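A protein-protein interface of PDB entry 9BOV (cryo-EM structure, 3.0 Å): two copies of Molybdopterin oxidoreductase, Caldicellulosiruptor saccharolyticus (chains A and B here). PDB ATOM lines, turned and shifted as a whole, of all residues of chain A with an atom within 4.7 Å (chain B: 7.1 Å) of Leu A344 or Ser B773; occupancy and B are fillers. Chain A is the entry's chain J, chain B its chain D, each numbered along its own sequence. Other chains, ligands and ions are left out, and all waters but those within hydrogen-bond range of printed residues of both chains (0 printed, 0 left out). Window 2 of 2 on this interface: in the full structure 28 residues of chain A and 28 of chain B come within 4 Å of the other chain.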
ATOM      1  N   PHE A 309      -0.909  28.662  15.456  1.00  0.00           N
ATOM      2  CA  PHE A 309       0.508  28.572  15.119  1.00  0.00           C
ATOM      3  C   PHE A 309       0.706  28.370  13.623  1.00  0.00           C
ATOM      4  O   PHE A 309       1.575  29.004  13.011  1.00  0.00           O
ATOM      5  CB  PHE A 309       1.153  27.435  15.912  1.00  0.00           C
ATOM      6  CG  PHE A 309       2.440  26.934  15.329  1.00  0.00           C
ATOM      7  CD1 PHE A 309       3.596  27.686  15.414  1.00  0.00           C
ATOM      8  CD2 PHE A 309       2.500  25.698  14.713  1.00  0.00           C
ATOM      9  CE1 PHE A 309       4.781  27.220  14.885  1.00  0.00           C
ATOM     10  CE2 PHE A 309       3.682  25.227  14.184  1.00  0.00           C
ATOM     11  CZ  PHE A 309       4.823  25.989  14.270  1.00  0.00           C
ATOM     12  N   VAL A 313       2.493  30.856  10.945  1.00  0.00           N
ATOM     13  CA  VAL A 313       3.567  30.384  10.074  1.00  0.00           C
ATOM     14  C   VAL A 313       3.239  30.680   8.616  1.00  0.00           C
ATOM     15  O   VAL A 313       4.085  31.163   7.856  1.00  0.00           O
ATOM     16  CB  VAL A 313       3.820  28.883  10.301  1.00  0.00           C
ATOM     17  CG1 VAL A 313       4.575  28.292   9.129  1.00  0.00           C
ATOM     18  CG2 VAL A 313       4.586  28.671  11.591  1.00  0.00           C
ATOM     19  N   VAL A 319       6.800  33.767  15.038  1.00  0.00           N
ATOM     20  CA  VAL A 319       6.375  32.883  16.114  1.00  0.00           C
ATOM     21  C   VAL A 319       7.553  32.677  17.053  1.00  0.00           C
ATOM     22  O   VAL A 319       8.717  32.785  16.655  1.00  0.00           O
ATOM     23  CB  VAL A 319       5.845  31.532  15.587  1.00  0.00           C
ATOM     24  CG1 VAL A 319       4.878  31.758  14.445  1.00  0.00           C
ATOM     25  CG2 VAL A 319       6.989  30.643  15.139  1.00  0.00           C
ATOM     26  N   LEU A 321       9.211  30.068  18.727  1.00  0.00           N
ATOM     27  CA  LEU A 321       9.525  28.656  18.863  1.00  0.00           C
ATOM     28  C   LEU A 321      10.724  28.495  19.795  1.00  0.00           C
ATOM     29  O   LEU A 321      11.154  29.440  20.461  1.00  0.00           O
ATOM     30  CB  LEU A 321       9.779  28.036  17.491  1.00  0.00           C
ATOM     31  CG  LEU A 321       9.023  26.747  17.170  1.00  0.00           C
ATOM     32  CD1 LEU A 321       7.527  26.966  17.274  1.00  0.00           C
ATOM     33  CD2 LEU A 321       9.395  26.247  15.789  1.00  0.00           C
ATOM     34  N   THR A 340       6.134  21.393  10.613  1.00  0.00           N
ATOM     35  CA  THR A 340       6.485  22.803  10.471  1.00  0.00           C
ATOM     36  C   THR A 340       7.541  23.212  11.488  1.00  0.00           C
ATOM     37  O   THR A 340       8.498  23.920  11.152  1.00  0.00           O
ATOM     38  CB  THR A 340       5.235  23.668  10.620  1.00  0.00           C
ATOM     39  OG1 THR A 340       4.343  23.414   9.529  1.00  0.00           O
ATOM     40  CG2 THR A 340       5.601  25.136  10.631  1.00  0.00           C
ATOM     41  N   ALA A 341       7.393  22.765  12.738  1.00  0.00           N
ATOM     42  CA  ALA A 341       8.393  23.058  13.756  1.00  0.00           C
ATOM     43  C   ALA A 341       9.735  22.437  13.402  1.00  0.00           C
ATOM     44  O   ALA A 341      10.787  23.042  13.630  1.00  0.00           O
ATOM     45  CB  ALA A 341       7.914  22.564  15.119  1.00  0.00           C
ATOM     46  N   ILE A 342       9.719  21.225  12.846  1.00  0.00           N
ATOM     47  CA  ILE A 342      10.958  20.605  12.386  1.00  0.00           C
ATOM     48  C   ILE A 342      11.607  21.455  11.302  1.00  0.00           C
ATOM     49  O   ILE A 342      12.824  21.675  11.309  1.00  0.00           O
ATOM     50  CB  ILE A 342      10.690  19.169  11.901  1.00  0.00           C
ATOM     51  CG1 ILE A 342      10.553  18.229  13.096  1.00  0.00           C
ATOM     52  CG2 ILE A 342      11.794  18.697  10.977  1.00  0.00           C
ATOM     53  CD1 ILE A 342      11.818  18.087  13.904  1.00  0.00           C
ATOM     54  N   ARG A 343      10.807  21.953  10.359  1.00  0.00           N
ATOM     55  CA  ARG A 343      11.341  22.798   9.299  1.00  0.00           C
ATOM     56  C   ARG A 343      11.633  24.221   9.754  1.00  0.00           C
ATOM     57  O   ARG A 343      12.351  24.938   9.051  1.00  0.00           O
ATOM     58  CB  ARG A 343      10.375  22.831   8.117  1.00  0.00           C
ATOM     59  CG  ARG A 343      10.154  21.479   7.484  1.00  0.00           C
ATOM     60  CD  ARG A 343       9.063  21.534   6.443  1.00  0.00           C
ATOM     61  NE  ARG A 343       9.214  20.481   5.448  1.00  0.00           N
ATOM     62  CZ  ARG A 343       8.938  19.206   5.669  1.00  0.00           C
ATOM     63  NH1 ARG A 343       8.498  18.788   6.843  1.00  0.00           N
ATOM     64  NH2 ARG A 343       9.104  18.326   4.686  1.00  0.00           N
ATOM     65  N   LEU A 344      11.105  24.645  10.899  1.00  0.00           N
ATOM     66  CA  LEU A 344      11.348  25.983  11.420  1.00  0.00           C
ATOM     67  C   LEU A 344      12.574  26.052  12.321  1.00  0.00           C
ATOM     68  O   LEU A 344      12.829  27.101  12.917  1.00  0.00           O
ATOM     69  CB  LEU A 344      10.121  26.493  12.178  1.00  0.00           C
ATOM     70  CG  LEU A 344       9.035  27.191  11.356  1.00  0.00           C
ATOM     71  CD1 LEU A 344       8.252  28.154  12.222  1.00  0.00           C
ATOM     72  CD2 LEU A 344       9.628  27.914  10.164  1.00  0.00           C
ATOM     73  N   GLY A 345      13.325  24.964  12.442  1.00  0.00           N
ATOM     74  CA  GLY A 345      14.576  24.977  13.167  1.00  0.00           C
ATOM     75  C   GLY A 345      14.559  24.368  14.550  1.00  0.00           C
ATOM     76  O   GLY A 345      15.571  24.456  15.253  1.00  0.00           O
ATOM     77  N   ALA A 346      13.451  23.761  14.968  1.00  0.00           N
ATOM     78  CA  ALA A 346      13.421  23.090  16.260  1.00  0.00           C
ATOM     79  C   ALA A 346      14.352  21.884  16.248  1.00  0.00           C
ATOM     80  O   ALA A 346      14.383  21.111  15.286  1.00  0.00           O
ATOM     81  CB  ALA A 346      11.999  22.659  16.605  1.00  0.00           C
ATOM     82  N   PHE A 544      10.495  24.361   2.903  1.00  0.00           N
ATOM     83  CA  PHE A 544       9.062  24.209   2.692  1.00  0.00           C
ATOM     84  C   PHE A 544       8.726  23.916   1.235  1.00  0.00           C
ATOM     85  O   PHE A 544       7.628  24.245   0.773  1.00  0.00           O
ATOM     86  CB  PHE A 544       8.321  25.455   3.171  1.00  0.00           C
ATOM     87  CG  PHE A 544       8.302  25.615   4.664  1.00  0.00           C
ATOM     88  CD1 PHE A 544       9.424  26.055   5.344  1.00  0.00           C
ATOM     89  CD2 PHE A 544       7.158  25.334   5.390  1.00  0.00           C
ATOM     90  CE1 PHE A 544       9.407  26.204   6.714  1.00  0.00           C
ATOM     91  CE2 PHE A 544       7.138  25.482   6.761  1.00  0.00           C
ATOM     92  CZ  PHE A 544       8.263  25.918   7.422  1.00  0.00           C
ATOM     93  N   LYS B 765      10.665  31.988   4.168  1.00  0.00           N
ATOM     94  CA  LYS B 765      10.616  30.884   5.121  1.00  0.00           C
ATOM     95  C   LYS B 765      11.929  30.740   5.879  1.00  0.00           C
ATOM     96  O   LYS B 765      11.923  30.432   7.073  1.00  0.00           O
ATOM     97  CB  LYS B 765      10.258  29.577   4.415  1.00  0.00           C
ATOM     98  CG  LYS B 765       8.968  29.629   3.618  1.00  0.00           C
ATOM     99  CD  LYS B 765       7.797  29.051   4.389  1.00  0.00           C
ATOM    100  CE  LYS B 765       7.007  30.133   5.094  1.00  0.00           C
ATOM    101  NZ  LYS B 765       5.606  29.710   5.346  1.00  0.00           N
ATOM    102  N   LYS B 766      13.066  30.960   5.212  1.00  0.00           N
ATOM    103  CA  LYS B 766      14.347  30.891   5.909  1.00  0.00           C
ATOM    104  C   LYS B 766      14.469  31.993   6.954  1.00  0.00           C
ATOM    105  O   LYS B 766      14.905  31.742   8.086  1.00  0.00           O
ATOM    106  CB  LYS B 766      15.493  30.971   4.904  1.00  0.00           C
ATOM    107  CG  LYS B 766      15.665  29.709   4.077  1.00  0.00           C
ATOM    108  CD  LYS B 766      16.846  29.809   3.131  1.00  0.00           C
ATOM    109  CE  LYS B 766      17.423  28.438   2.827  1.00  0.00           C
ATOM    110  NZ  LYS B 766      16.462  27.345   3.143  1.00  0.00           N
ATOM    111  N   LEU B 767      14.079  33.219   6.598  1.00  0.00           N
ATOM    112  CA  LEU B 767      14.117  34.309   7.567  1.00  0.00           C
ATOM    113  C   LEU B 767      13.179  34.037   8.736  1.00  0.00           C
ATOM    114  O   LEU B 767      13.533  34.282   9.897  1.00  0.00           O
ATOM    115  CB  LEU B 767      13.759  35.631   6.889  1.00  0.00           C
ATOM    116  CG  LEU B 767      14.736  36.136   5.830  1.00  0.00           C
ATOM    117  CD1 LEU B 767      14.273  37.466   5.271  1.00  0.00           C
ATOM    118  CD2 LEU B 767      16.137  36.253   6.403  1.00  0.00           C
ATOM    119  N   GLN B 768      11.981  33.521   8.452  1.00  0.00           N
ATOM    120  CA  GLN B 768      11.033  33.226   9.518  1.00  0.00           C
ATOM    121  C   GLN B 768      11.541  32.108  10.418  1.00  0.00           C
ATOM    122  O   GLN B 768      11.344  32.151  11.634  1.00  0.00           O
ATOM    123  CB  GLN B 768       9.673  32.864   8.928  1.00  0.00           C
ATOM    124  CG  GLN B 768       8.592  32.681   9.970  1.00  0.00           C
ATOM    125  CD  GLN B 768       7.553  31.666   9.558  1.00  0.00           C
ATOM    126  OE1 GLN B 768       7.501  31.250   8.402  1.00  0.00           O
ATOM    127  NE2 GLN B 768       6.723  31.254  10.505  1.00  0.00           N
ATOM    128  N   ALA B 769      12.189  31.097   9.839  1.00  0.00           N
ATOM    129  CA  ALA B 769      12.756  30.021  10.644  1.00  0.00           C
ATOM    130  C   ALA B 769      13.860  30.538  11.552  1.00  0.00           C
ATOM    131  O   ALA B 769      13.941  30.153  12.726  1.00  0.00           O
ATOM    132  CB  ALA B 769      13.282  28.910   9.739  1.00  0.00           C
ATOM    133  N   ILE B 770      14.723  31.410  11.027  1.00  0.00           N
ATOM    134  CA  ILE B 770      15.782  31.986  11.851  1.00  0.00           C
ATOM    135  C   ILE B 770      15.181  32.793  12.994  1.00  0.00           C
ATOM    136  O   ILE B 770      15.590  32.664  14.154  1.00  0.00           O
ATOM    137  CB  ILE B 770      16.729  32.842  10.992  1.00  0.00           C
ATOM    138  CG1 ILE B 770      17.632  31.947  10.142  1.00  0.00           C
ATOM    139  CG2 ILE B 770      17.564  33.750  11.872  1.00  0.00           C
ATOM    140  CD1 ILE B 770      18.710  31.248  10.931  1.00  0.00           C
ATOM    141  N   ARG B 771      14.184  33.626  12.684  1.00  0.00           N
ATOM    142  CA  ARG B 771      13.555  34.441  13.719  1.00  0.00           C
ATOM    143  C   ARG B 771      12.868  33.575  14.768  1.00  0.00           C
ATOM    144  O   ARG B 771      12.940  33.865  15.967  1.00  0.00           O
ATOM    145  CB  ARG B 771      12.561  35.413  13.085  1.00  0.00           C
ATOM    146  CG  ARG B 771      11.433  35.848  14.001  1.00  0.00           C
ATOM    147  CD  ARG B 771      11.906  36.861  15.027  1.00  0.00           C
ATOM    148  NE  ARG B 771      10.801  37.408  15.804  1.00  0.00           N
ATOM    149  CZ  ARG B 771      10.318  36.858  16.909  1.00  0.00           C
ATOM    150  NH1 ARG B 771      10.816  35.733  17.395  1.00  0.00           N
ATOM    151  NH2 ARG B 771       9.310  37.451  17.543  1.00  0.00           N
ATOM    152  N   ALA B 772      12.202  32.503  14.337  1.00  0.00           N
ATOM    153  CA  ALA B 772      11.494  31.637  15.272  1.00  0.00           C
ATOM    154  C   ALA B 772      12.461  30.901  16.187  1.00  0.00           C
ATOM    155  O   ALA B 772      12.275  30.874  17.408  1.00  0.00           O
ATOM    156  CB  ALA B 772      10.620  30.644  14.505  1.00  0.00           C
ATOM    157  N   SER B 773      13.503  30.296  15.617  1.00  0.00           N
ATOM    158  CA  SER B 773      14.407  29.489  16.428  1.00  0.00           C
ATOM    159  C   SER B 773      15.285  30.353  17.326  1.00  0.00           C
ATOM    160  O   SER B 773      15.492  30.022  18.499  1.00  0.00           O
ATOM    161  CB  SER B 773      15.267  28.601  15.530  1.00  0.00           C
ATOM    162  OG  SER B 773      15.571  29.249  14.309  1.00  0.00           O
ATOM    163  N   TYR B 774      15.803  31.468  16.807  1.00  0.00           N
ATOM    164  CA  TYR B 774      16.791  32.260  17.524  1.00  0.00           C
ATOM    165  C   TYR B 774      16.248  33.568  18.082  1.00  0.00           C
ATOM    166  O   TYR B 774      17.023  34.354  18.635  1.00  0.00           O
ATOM    167  CB  TYR B 774      17.990  32.544  16.614  1.00  0.00           C
ATOM    168  CG  TYR B 774      18.729  31.298  16.195  1.00  0.00           C
ATOM    169  CD1 TYR B 774      19.593  30.655  17.067  1.00  0.00           C
ATOM    170  CD2 TYR B 774      18.560  30.760  14.929  1.00  0.00           C
ATOM    171  CE1 TYR B 774      20.269  29.514  16.690  1.00  0.00           C
ATOM    172  CE2 TYR B 774      19.232  29.620  14.542  1.00  0.00           C
ATOM    173  CZ  TYR B 774      20.085  29.002  15.427  1.00  0.00           C
ATOM    174  OH  TYR B 774      20.757  27.865  15.045  1.00  0.00           O
ATOM    175  N   GLY B 775      14.953  33.826  17.961  1.00  0.00           N
ATOM    176  CA  GLY B 775      14.372  35.001  18.570  1.00  0.00           C
ATOM    177  C   GLY B 775      14.635  36.277  17.791  1.00  0.00           C
ATOM    178  O   GLY B 775      15.160  36.280  16.675  1.00  0.00           O
ATOM    179  N   SER B 778      17.969  38.656  15.456  1.00  0.00           N
ATOM    180  CA  SER B 778      18.879  37.611  15.012  1.00  0.00           C
ATOM    181  C   SER B 778      19.121  37.629  13.511  1.00  0.00           C
ATOM    182  O   SER B 778      19.868  36.783  13.010  1.00  0.00           O
ATOM    183  CB  SER B 778      18.350  36.235  15.428  1.00  0.00           C
ATOM    184  OG  SER B 778      16.960  36.134  15.182  1.00  0.00           O
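OG of Ser B773 sits at hydrogen-bond distance from O of Ala B769 (2.4 Å). OG of Ser B773 is in hydrogen-bond range of O of Ile B770, at 3.4 Å.
Of the printed residues of chain B, Val A319 touches Arg B771 and Ala B772. Ala A341 touches none of the printed residues of chain B. Of chain B, only Gln B768, Ala B769 and Ser B773 come within 4 Å of Leu A344. Of the printed residues of chain A, Gln B768 touches Val A313 (3.3 Å) and Leu A344 (3.9 Å). Of the printed residues of chain A, Ala B772 touches Val A319 (3.3 Å) and Leu A321 (3.4 Å). Tyr B774 touches none of the printed residues of chain A. The nearest residue of chain A that does not touch Ser B773 is Gly A345 (4.2 Å).
Among the printed residues, pairs that only touch across the chains: Val A319 with Arg B771, Val A319 with Ala B772, Leu A344 with Gln B768, Leu A344 with Ser B773 and Phe A544 with Lys B765.
Hydrophobic or aromatic side chains of chain A within 4 Å of the printed part of chain B: Val A313, Val A319, Leu A321, Leu A344 and Phe A544. Of the 12 printed residues of chain B, 6 touch a printed residue of chain A. Printed residues of chain B that touch a printed residue of chain A: Lys B765, Gln B768, Ala B769, Arg B771, Ala B772 and Ser B773. Among the printed residues, 9 pairs touch across the chains.
The backbone carbonyl oxygen (O) of Val A313 lies within hydrogen-bond range of the side-chain amino group (NZ) of Lys B765 (3.3 Å). The backbone carbonyl oxygen (O) of Val A313 lies close to the side-chain amide oxygen (OE1) of Gln B768. The backbone carbonyl oxygen of Ala B772 lies within hydrogen-bond range of the backbone NH of Leu A321, 3.4 Å away. The backbone carbonyl oxygen of Leu A344 sits close to the backbone carbonyl oxygen of Ala B769, at 3.3 Å.
No position is printed for both chains.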
